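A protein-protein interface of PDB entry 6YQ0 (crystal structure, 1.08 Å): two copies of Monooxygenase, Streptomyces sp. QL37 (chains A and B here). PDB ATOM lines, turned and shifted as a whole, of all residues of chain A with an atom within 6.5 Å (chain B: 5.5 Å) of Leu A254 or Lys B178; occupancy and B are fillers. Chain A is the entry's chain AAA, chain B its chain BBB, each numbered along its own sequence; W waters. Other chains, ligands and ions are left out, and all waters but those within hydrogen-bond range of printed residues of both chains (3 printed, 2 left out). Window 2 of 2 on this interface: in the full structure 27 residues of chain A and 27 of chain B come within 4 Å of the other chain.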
ATOM      1  N   GLN A 213      18.166   0.014 -17.824  1.00  0.00           N
ATOM      2  CA  GLN A 213      18.486   1.147 -18.712  1.00  0.00           C
ATOM      3  C   GLN A 213      19.984   1.123 -19.077  1.00  0.00           C
ATOM      4  O   GLN A 213      20.257   1.721 -20.066  1.00  0.00           O
ATOM      5  CB  GLN A 213      17.994   2.457 -18.082  1.00  0.00           C
ATOM      6  CG  GLN A 213      16.503   2.510 -17.728  1.00  0.00           C
ATOM      7  CD  GLN A 213      15.624   2.010 -18.843  1.00  0.00           C
ATOM      8  OE1 GLN A 213      15.647   2.573 -19.941  1.00  0.00           O
ATOM      9  NE2 GLN A 213      14.890   0.923 -18.643  1.00  0.00           N
ATOM     10  N   SER A 214      20.847   0.463 -18.289  1.00  0.00           N
ATOM     11  CA  SER A 214      22.310   0.406 -18.534  1.00  0.00           C
ATOM     12  C   SER A 214      22.621  -0.346 -19.855  1.00  0.00           C
ATOM     13  O   SER A 214      23.582  -0.001 -20.527  1.00  0.00           O
ATOM     14  CB  SER A 214      23.051  -0.159 -17.348  1.00  0.00           C
ATOM     15  OG  SER A 214      22.606  -1.512 -17.047  1.00  0.00           O
ATOM     16  N   SER A 215      21.761  -1.238 -20.210  1.00  0.00           N
ATOM     17  CA  SER A 215      21.970  -2.078 -21.438  1.00  0.00           C
ATOM     18  C   SER A 215      21.400  -1.390 -22.675  1.00  0.00           C
ATOM     19  O   SER A 215      20.302  -0.835 -22.629  1.00  0.00           O
ATOM     20  CB  SER A 215      21.366  -3.423 -21.240  1.00  0.00           C
ATOM     21  OG  SER A 215      21.168  -4.077 -22.505  1.00  0.00           O
ATOM     22  N   ALA A 216      22.067  -1.500 -23.839  1.00  0.00           N
ATOM     23  CA  ALA A 216      21.517  -1.053 -25.108  1.00  0.00           C
ATOM     24  C   ALA A 216      20.221  -1.783 -25.455  1.00  0.00           C
ATOM     25  O   ALA A 216      19.391  -1.248 -26.188  1.00  0.00           O
ATOM     26  CB  ALA A 216      22.549  -1.250 -26.172  1.00  0.00           C
ATOM     27  N   LYS A 218      18.042  -2.663 -23.171  1.00  0.00           N
ATOM     28  CA  LYS A 218      16.991  -2.180 -22.209  1.00  0.00           C
ATOM     29  C   LYS A 218      16.373  -3.381 -21.465  1.00  0.00           C
ATOM     30  O   LYS A 218      15.146  -3.393 -21.179  1.00  0.00           O
ATOM     31  CB  LYS A 218      15.963  -1.297 -22.882  1.00  0.00           C
ATOM     32  CG  LYS A 218      16.548  -0.028 -23.513  1.00  0.00           C
ATOM     33  CD  LYS A 218      17.276   0.861 -22.557  1.00  0.00           C
ATOM     34  CE  LYS A 218      18.191   1.828 -23.289  1.00  0.00           C
ATOM     35  NZ  LYS A 218      18.845   2.810 -22.407  1.00  0.00           N
ATOM     36  N   ASP A 247      33.300  -8.896 -23.943  1.00  0.00           N
ATOM     37  CA  ASP A 247      32.159  -8.147 -23.416  1.00  0.00           C
ATOM     38  C   ASP A 247      30.904  -8.988 -23.478  1.00  0.00           C
ATOM     39  O   ASP A 247      30.418  -9.331 -24.619  1.00  0.00           O
ATOM     40  CB  ASP A 247      32.023  -6.892 -24.259  1.00  0.00           C
ATOM     41  CG  ASP A 247      30.945  -5.985 -23.906  1.00  0.00           C
ATOM     42  OD1 ASP A 247      29.891  -6.430 -23.387  1.00  0.00           O
ATOM     43  OD2 ASP A 247      31.024  -4.766 -24.319  1.00  0.00           O
ATOM     44  N   SER A 249      27.970  -8.086 -21.825  1.00  0.00           N
ATOM     45  CA  SER A 249      27.220  -7.107 -21.008  1.00  0.00           C
ATOM     46  C   SER A 249      25.923  -6.689 -21.631  1.00  0.00           C
ATOM     47  O   SER A 249      25.295  -5.729 -21.095  1.00  0.00           O
ATOM     48  CB  SER A 249      28.064  -5.886 -20.735  1.00  0.00           C
ATOM     49  OG  SER A 249      28.177  -5.009 -21.860  1.00  0.00           O
ATOM     50  N   GLY A 250      25.529  -7.213 -22.745  1.00  0.00           N
ATOM     51  CA  GLY A 250      24.328  -6.700 -23.378  1.00  0.00           C
ATOM     52  C   GLY A 250      24.494  -5.253 -23.843  1.00  0.00           C
ATOM     53  O   GLY A 250      23.507  -4.438 -23.716  1.00  0.00           O
ATOM     54  N   GLY A 251      25.611  -4.869 -24.352  1.00  0.00           N
ATOM     55  CA  GLY A 251      25.706  -3.517 -24.891  1.00  0.00           C
ATOM     56  C   GLY A 251      25.743  -2.490 -23.758  1.00  0.00           C
ATOM     57  O   GLY A 251      25.163  -1.405 -23.966  1.00  0.00           O
ATOM     58  N   THR A 252      26.261  -2.775 -22.622  1.00  0.00           N
ATOM     59  CA  THR A 252      26.371  -1.780 -21.531  1.00  0.00           C
ATOM     60  C   THR A 252      27.709  -1.015 -21.680  1.00  0.00           C
ATOM     61  O   THR A 252      27.886  -0.032 -20.893  1.00  0.00           O
ATOM     62  CB  THR A 252      26.366  -2.513 -20.189  1.00  0.00           C
ATOM     63  OG1 THR A 252      25.230  -3.354 -20.064  1.00  0.00           O
ATOM     64  CG2 THR A 252      26.553  -1.650 -19.002  1.00  0.00           C
ATOM     65  N   LEU A 253      28.634  -1.402 -22.467  1.00  0.00           N
ATOM     66  CA  LEU A 253      30.033  -0.854 -22.585  1.00  0.00           C
ATOM     67  C   LEU A 253      30.114  -0.068 -23.868  1.00  0.00           C
ATOM     68  O   LEU A 253      31.221  -0.163 -24.542  1.00  0.00           O
ATOM     69  CB  LEU A 253      31.090  -1.934 -22.441  1.00  0.00           C
ATOM     70  CG  LEU A 253      30.974  -2.744 -21.148  1.00  0.00           C
ATOM     71  CD1 LEU A 253      32.117  -3.780 -21.044  1.00  0.00           C
ATOM     72  CD2 LEU A 253      30.960  -1.910 -19.948  1.00  0.00           C
ATOM     73  N   LEU A 254      29.069   0.641 -24.234  1.00  0.00           N
ATOM     74  CA  LEU A 254      29.113   1.491 -25.448  1.00  0.00           C
ATOM     75  C   LEU A 254      29.462   2.914 -25.068  1.00  0.00           C
ATOM     76  O   LEU A 254      29.562   3.759 -26.004  1.00  0.00           O
ATOM     77  CB  LEU A 254      27.769   1.373 -26.212  1.00  0.00           C
ATOM     78  CG  LEU A 254      27.315  -0.035 -26.598  1.00  0.00           C
ATOM     79  CD1 LEU A 254      26.046  -0.052 -27.339  1.00  0.00           C
ATOM     80  CD2 LEU A 254      28.337  -0.777 -27.299  1.00  0.00           C
ATOM     81  N   GLY A 255      29.831   3.220 -23.827  1.00  0.00           N
ATOM     82  CA  GLY A 255      30.192   4.584 -23.361  1.00  0.00           C
ATOM     83  C   GLY A 255      28.971   5.358 -22.957  1.00  0.00           C
ATOM     84  O   GLY A 255      29.258   6.432 -22.324  1.00  0.00           O
ATOM     85  N   THR B 173      31.076  -0.502 -35.964  1.00  0.00           N
ATOM     86  CA  THR B 173      30.677  -1.419 -34.898  1.00  0.00           C
ATOM     87  C   THR B 173      30.120  -0.674 -33.704  1.00  0.00           C
ATOM     88  O   THR B 173      29.024  -0.987 -33.214  1.00  0.00           O
ATOM     89  CB  THR B 173      31.839  -2.293 -34.480  1.00  0.00           C
ATOM     90  OG1 THR B 173      32.142  -3.159 -35.608  1.00  0.00           O
ATOM     91  CG2 THR B 173      31.498  -3.102 -33.259  1.00  0.00           C
ATOM     92  N   LEU B 174      30.853   0.293 -33.178  1.00  0.00           N
ATOM     93  CA  LEU B 174      30.457   0.974 -31.926  1.00  0.00           C
ATOM     94  C   LEU B 174      29.107   1.646 -32.070  1.00  0.00           C
ATOM     95  O   LEU B 174      28.167   1.451 -31.284  1.00  0.00           O
ATOM     96  CB  LEU B 174      31.551   1.947 -31.523  1.00  0.00           C
ATOM     97  CG  LEU B 174      31.278   2.772 -30.300  1.00  0.00           C
ATOM     98  CD1 LEU B 174      31.020   1.977 -29.049  1.00  0.00           C
ATOM     99  CD2 LEU B 174      32.399   3.771 -30.058  1.00  0.00           C
ATOM    100  N   HIS B 175      29.008   2.520 -33.099  1.00  0.00           N
ATOM    101  CA  HIS B 175      27.843   3.384 -33.172  1.00  0.00           C
ATOM    102  C   HIS B 175      26.636   2.634 -33.717  1.00  0.00           C
ATOM    103  O   HIS B 175      25.499   2.881 -33.272  1.00  0.00           O
ATOM    104  CB  HIS B 175      28.186   4.638 -33.991  1.00  0.00           C
ATOM    105  CG  HIS B 175      29.252   5.443 -33.362  1.00  0.00           C
ATOM    106  ND1 HIS B 175      28.990   6.286 -32.297  1.00  0.00           N
ATOM    107  CD2 HIS B 175      30.582   5.419 -33.551  1.00  0.00           C
ATOM    108  CE1 HIS B 175      30.163   6.738 -31.903  1.00  0.00           C
ATOM    109  NE2 HIS B 175      31.175   6.234 -32.639  1.00  0.00           N
ATOM    110  N   MET B 176      26.847   1.721 -34.664  1.00  0.00           N
ATOM    111  CA  MET B 176      25.698   0.956 -35.172  1.00  0.00           C
ATOM    112  C   MET B 176      25.231  -0.077 -34.158  1.00  0.00           C
ATOM    113  O   MET B 176      24.028  -0.394 -34.153  1.00  0.00           O
ATOM    114  CB  MET B 176      25.994   0.276 -36.491  1.00  0.00           C
ATOM    115  CG  MET B 176      26.271   1.295 -37.637  1.00  0.00           C
ATOM    116  SD  MET B 176      24.964   2.480 -37.915  1.00  0.00           S
ATOM    117  CE  MET B 176      23.702   1.436 -38.597  1.00  0.00           C
ATOM    118  N   ALA B 177      26.072  -0.583 -33.261  1.00  0.00           N
ATOM    119  CA  ALA B 177      25.589  -1.469 -32.195  1.00  0.00           C
ATOM    120  C   ALA B 177      24.545  -0.755 -31.380  1.00  0.00           C
ATOM    121  O   ALA B 177      23.488  -1.317 -31.051  1.00  0.00           O
ATOM    122  CB  ALA B 177      26.740  -1.968 -31.329  1.00  0.00           C
ATOM    123  N   LYS B 178      24.792   0.505 -31.015  1.00  0.00           N
ATOM    124  CA  LYS B 178      23.794   1.248 -30.231  1.00  0.00           C
ATOM    125  C   LYS B 178      22.551   1.485 -31.086  1.00  0.00           C
ATOM    126  O   LYS B 178      21.415   1.316 -30.592  1.00  0.00           O
ATOM    127  CB  LYS B 178      24.429   2.564 -29.790  1.00  0.00           C
ATOM    128  CG  LYS B 178      23.536   3.490 -29.017  1.00  0.00           C
ATOM    129  CD  LYS B 178      23.063   2.882 -27.761  1.00  0.00           C
ATOM    130  CE  LYS B 178      22.111   3.815 -27.008  1.00  0.00           C
ATOM    131  NZ  LYS B 178      21.770   3.329 -25.637  1.00  0.00           N
ATOM    132  N   HIS B 179      22.734   1.882 -32.326  1.00  0.00           N
ATOM    133  CA  HIS B 179      21.581   2.203 -33.206  1.00  0.00           C
ATOM    134  C   HIS B 179      20.650   1.010 -33.374  1.00  0.00           C
ATOM    135  O   HIS B 179      19.432   1.227 -33.428  1.00  0.00           O
ATOM    136  CB  HIS B 179      22.087   2.691 -34.523  1.00  0.00           C
ATOM    137  CG  HIS B 179      21.020   3.233 -35.398  1.00  0.00           C
ATOM    138  ND1 HIS B 179      20.307   4.310 -35.063  1.00  0.00           N
ATOM    139  CD2 HIS B 179      20.547   2.764 -36.548  1.00  0.00           C
ATOM    140  CE1 HIS B 179      19.401   4.466 -36.085  1.00  0.00           C
ATOM    141  NE2 HIS B 179      19.538   3.679 -36.895  1.00  0.00           N
ATOM    142  N   LEU B 180      21.232  -0.163 -33.571  1.00  0.00           N
ATOM    143  CA  LEU B 180      20.458  -1.344 -33.993  1.00  0.00           C
ATOM    144  C   LEU B 180      20.013  -2.202 -32.817  1.00  0.00           C
ATOM    145  O   LEU B 180      19.234  -3.139 -32.979  1.00  0.00           O
ATOM    146  CB  LEU B 180      21.263  -2.142 -34.985  1.00  0.00           C
ATOM    147  CG  LEU B 180      21.515  -1.424 -36.319  1.00  0.00           C
ATOM    148  CD1 LEU B 180      22.450  -2.240 -37.152  1.00  0.00           C
ATOM    149  CD2 LEU B 180      20.223  -1.132 -37.080  1.00  0.00           C
ATOM    150  N   ALA B 181      20.474  -1.895 -31.608  1.00  0.00           N
ATOM    151  CA  ALA B 181      20.135  -2.670 -30.410  1.00  0.00           C
ATOM    152  C   ALA B 181      18.606  -2.787 -30.226  1.00  0.00           C
ATOM    153  O   ALA B 181      18.156  -3.867 -29.827  1.00  0.00           O
ATOM    154  CB  ALA B 181      20.771  -2.094 -29.165  1.00  0.00           C
ATOM    155  N   PRO B 182      17.792  -1.758 -30.470  1.00  0.00           N
ATOM    156  CA  PRO B 182      16.351  -1.891 -30.285  1.00  0.00           C
ATOM    157  C   PRO B 182      15.756  -2.956 -31.184  1.00  0.00           C
ATOM    158  O   PRO B 182      14.640  -3.437 -30.861  1.00  0.00           O
ATOM    159  CB  PRO B 182      15.760  -0.497 -30.569  1.00  0.00           C
ATOM    160  CG  PRO B 182      16.942   0.437 -30.287  1.00  0.00           C
ATOM    161  CD  PRO B 182      18.152  -0.350 -30.772  1.00  0.00           C
ATOM    162  N   THR B 242      27.461  -7.216 -28.001  1.00  0.00           N
ATOM    163  CA  THR B 242      27.256  -6.245 -29.089  1.00  0.00           C
ATOM    164  C   THR B 242      28.153  -5.063 -28.845  1.00  0.00           C
ATOM    165  O   THR B 242      28.475  -4.717 -27.693  1.00  0.00           O
ATOM    166  CB  THR B 242      25.787  -5.811 -29.220  1.00  0.00           C
ATOM    167  OG1 THR B 242      25.671  -5.255 -30.544  1.00  0.00           O
ATOM    168  CG2 THR B 242      25.301  -4.872 -28.160  1.00  0.00           C
ATOM    169  N   GLY B 243      28.576  -4.445 -29.928  1.00  0.00           N
ATOM    170  CA  GLY B 243      29.497  -3.334 -29.877  1.00  0.00           C
ATOM    171  C   GLY B 243      30.895  -3.706 -29.482  1.00  0.00           C
ATOM    172  O   GLY B 243      31.648  -2.787 -29.105  1.00  0.00           O
HETATM  173  O   HOH W   1      32.359  -1.392 -26.801  1.00  0.00           O
HETATM  174  O   HOH W   2      19.958   1.318 -26.746  1.00  0.00           O
HETATM  175  O   HOH W   3      28.874  -3.334 -24.869  1.00  0.00           O
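O of Gly A250 sits at hydrogen-bond distance from N of Ala A216. N of Ala A216 lies within hydrogen-bond range of O of Gly A251 (3.1 Å).
Ala B181 touches Ala A216. Thr B242 touches Gly A251. Leu B174 touches Leu A254 (CD1 to O, 3.8 Å). Leu A254 touches Lys B178 (CD1 to CA, 3.9 Å). CD2 of Leu A254 touches O of Thr B242 (3.96 Å). Leu A254 touches Gly B243 (CD2 to CA, 3.8 Å).
Of the printed residues of chain B, Ala A216 touches Ala B181 (3.4 Å). Asp A247 touches none of the printed residues of chain B. Of the printed residues of chain B, Gly A251 touches Thr B242. Printed residues of chain B within 4 Å of Leu A254: Leu B174 (3.8 Å), Lys B178 (3.9 Å), Thr B242 (3.96 Å) and Gly B243 (3.8 Å). Printed residues of chain A within 4 Å of Lys B178: Leu A254. Of the printed residues of chain A, Ala B181 touches Ala A216.
Of the 12 printed residues of chain B, 5 touch a printed residue of chain A. Hydrophobic or aromatic side chains of chain A that line the printed part of chain B: Ala A216 and Leu A254. Among the printed residues, 6 pairs touch across the chains. Among the printed residues, no Asp or Glu carboxylate lies within 4 Å of a Lys or Arg side-chain nitrogen of the other chain.
No position is printed for both chains. Of the 6 pairs that touch across the chains among the printed residues, none has its exchanged pair printed and touching as well.
Water W3 lies within hydrogen-bond range of OD2 of Asp A247 (2.6 Å), N of Leu A253 (3.1 Å), O of Thr B242 (3.2 Å) and N of Thr A252 (3.5 Å). Water W2 lies within hydrogen-bond range of the backbone carbonyl oxygen of Ala A216 (2.7 Å) and the side-chain amino group of Lys B178 (2.9 Å). Water W1 lies within hydrogen-bond range of O of Gly B243 (2.8 Å) and O of Leu A253 (2.8 Å).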
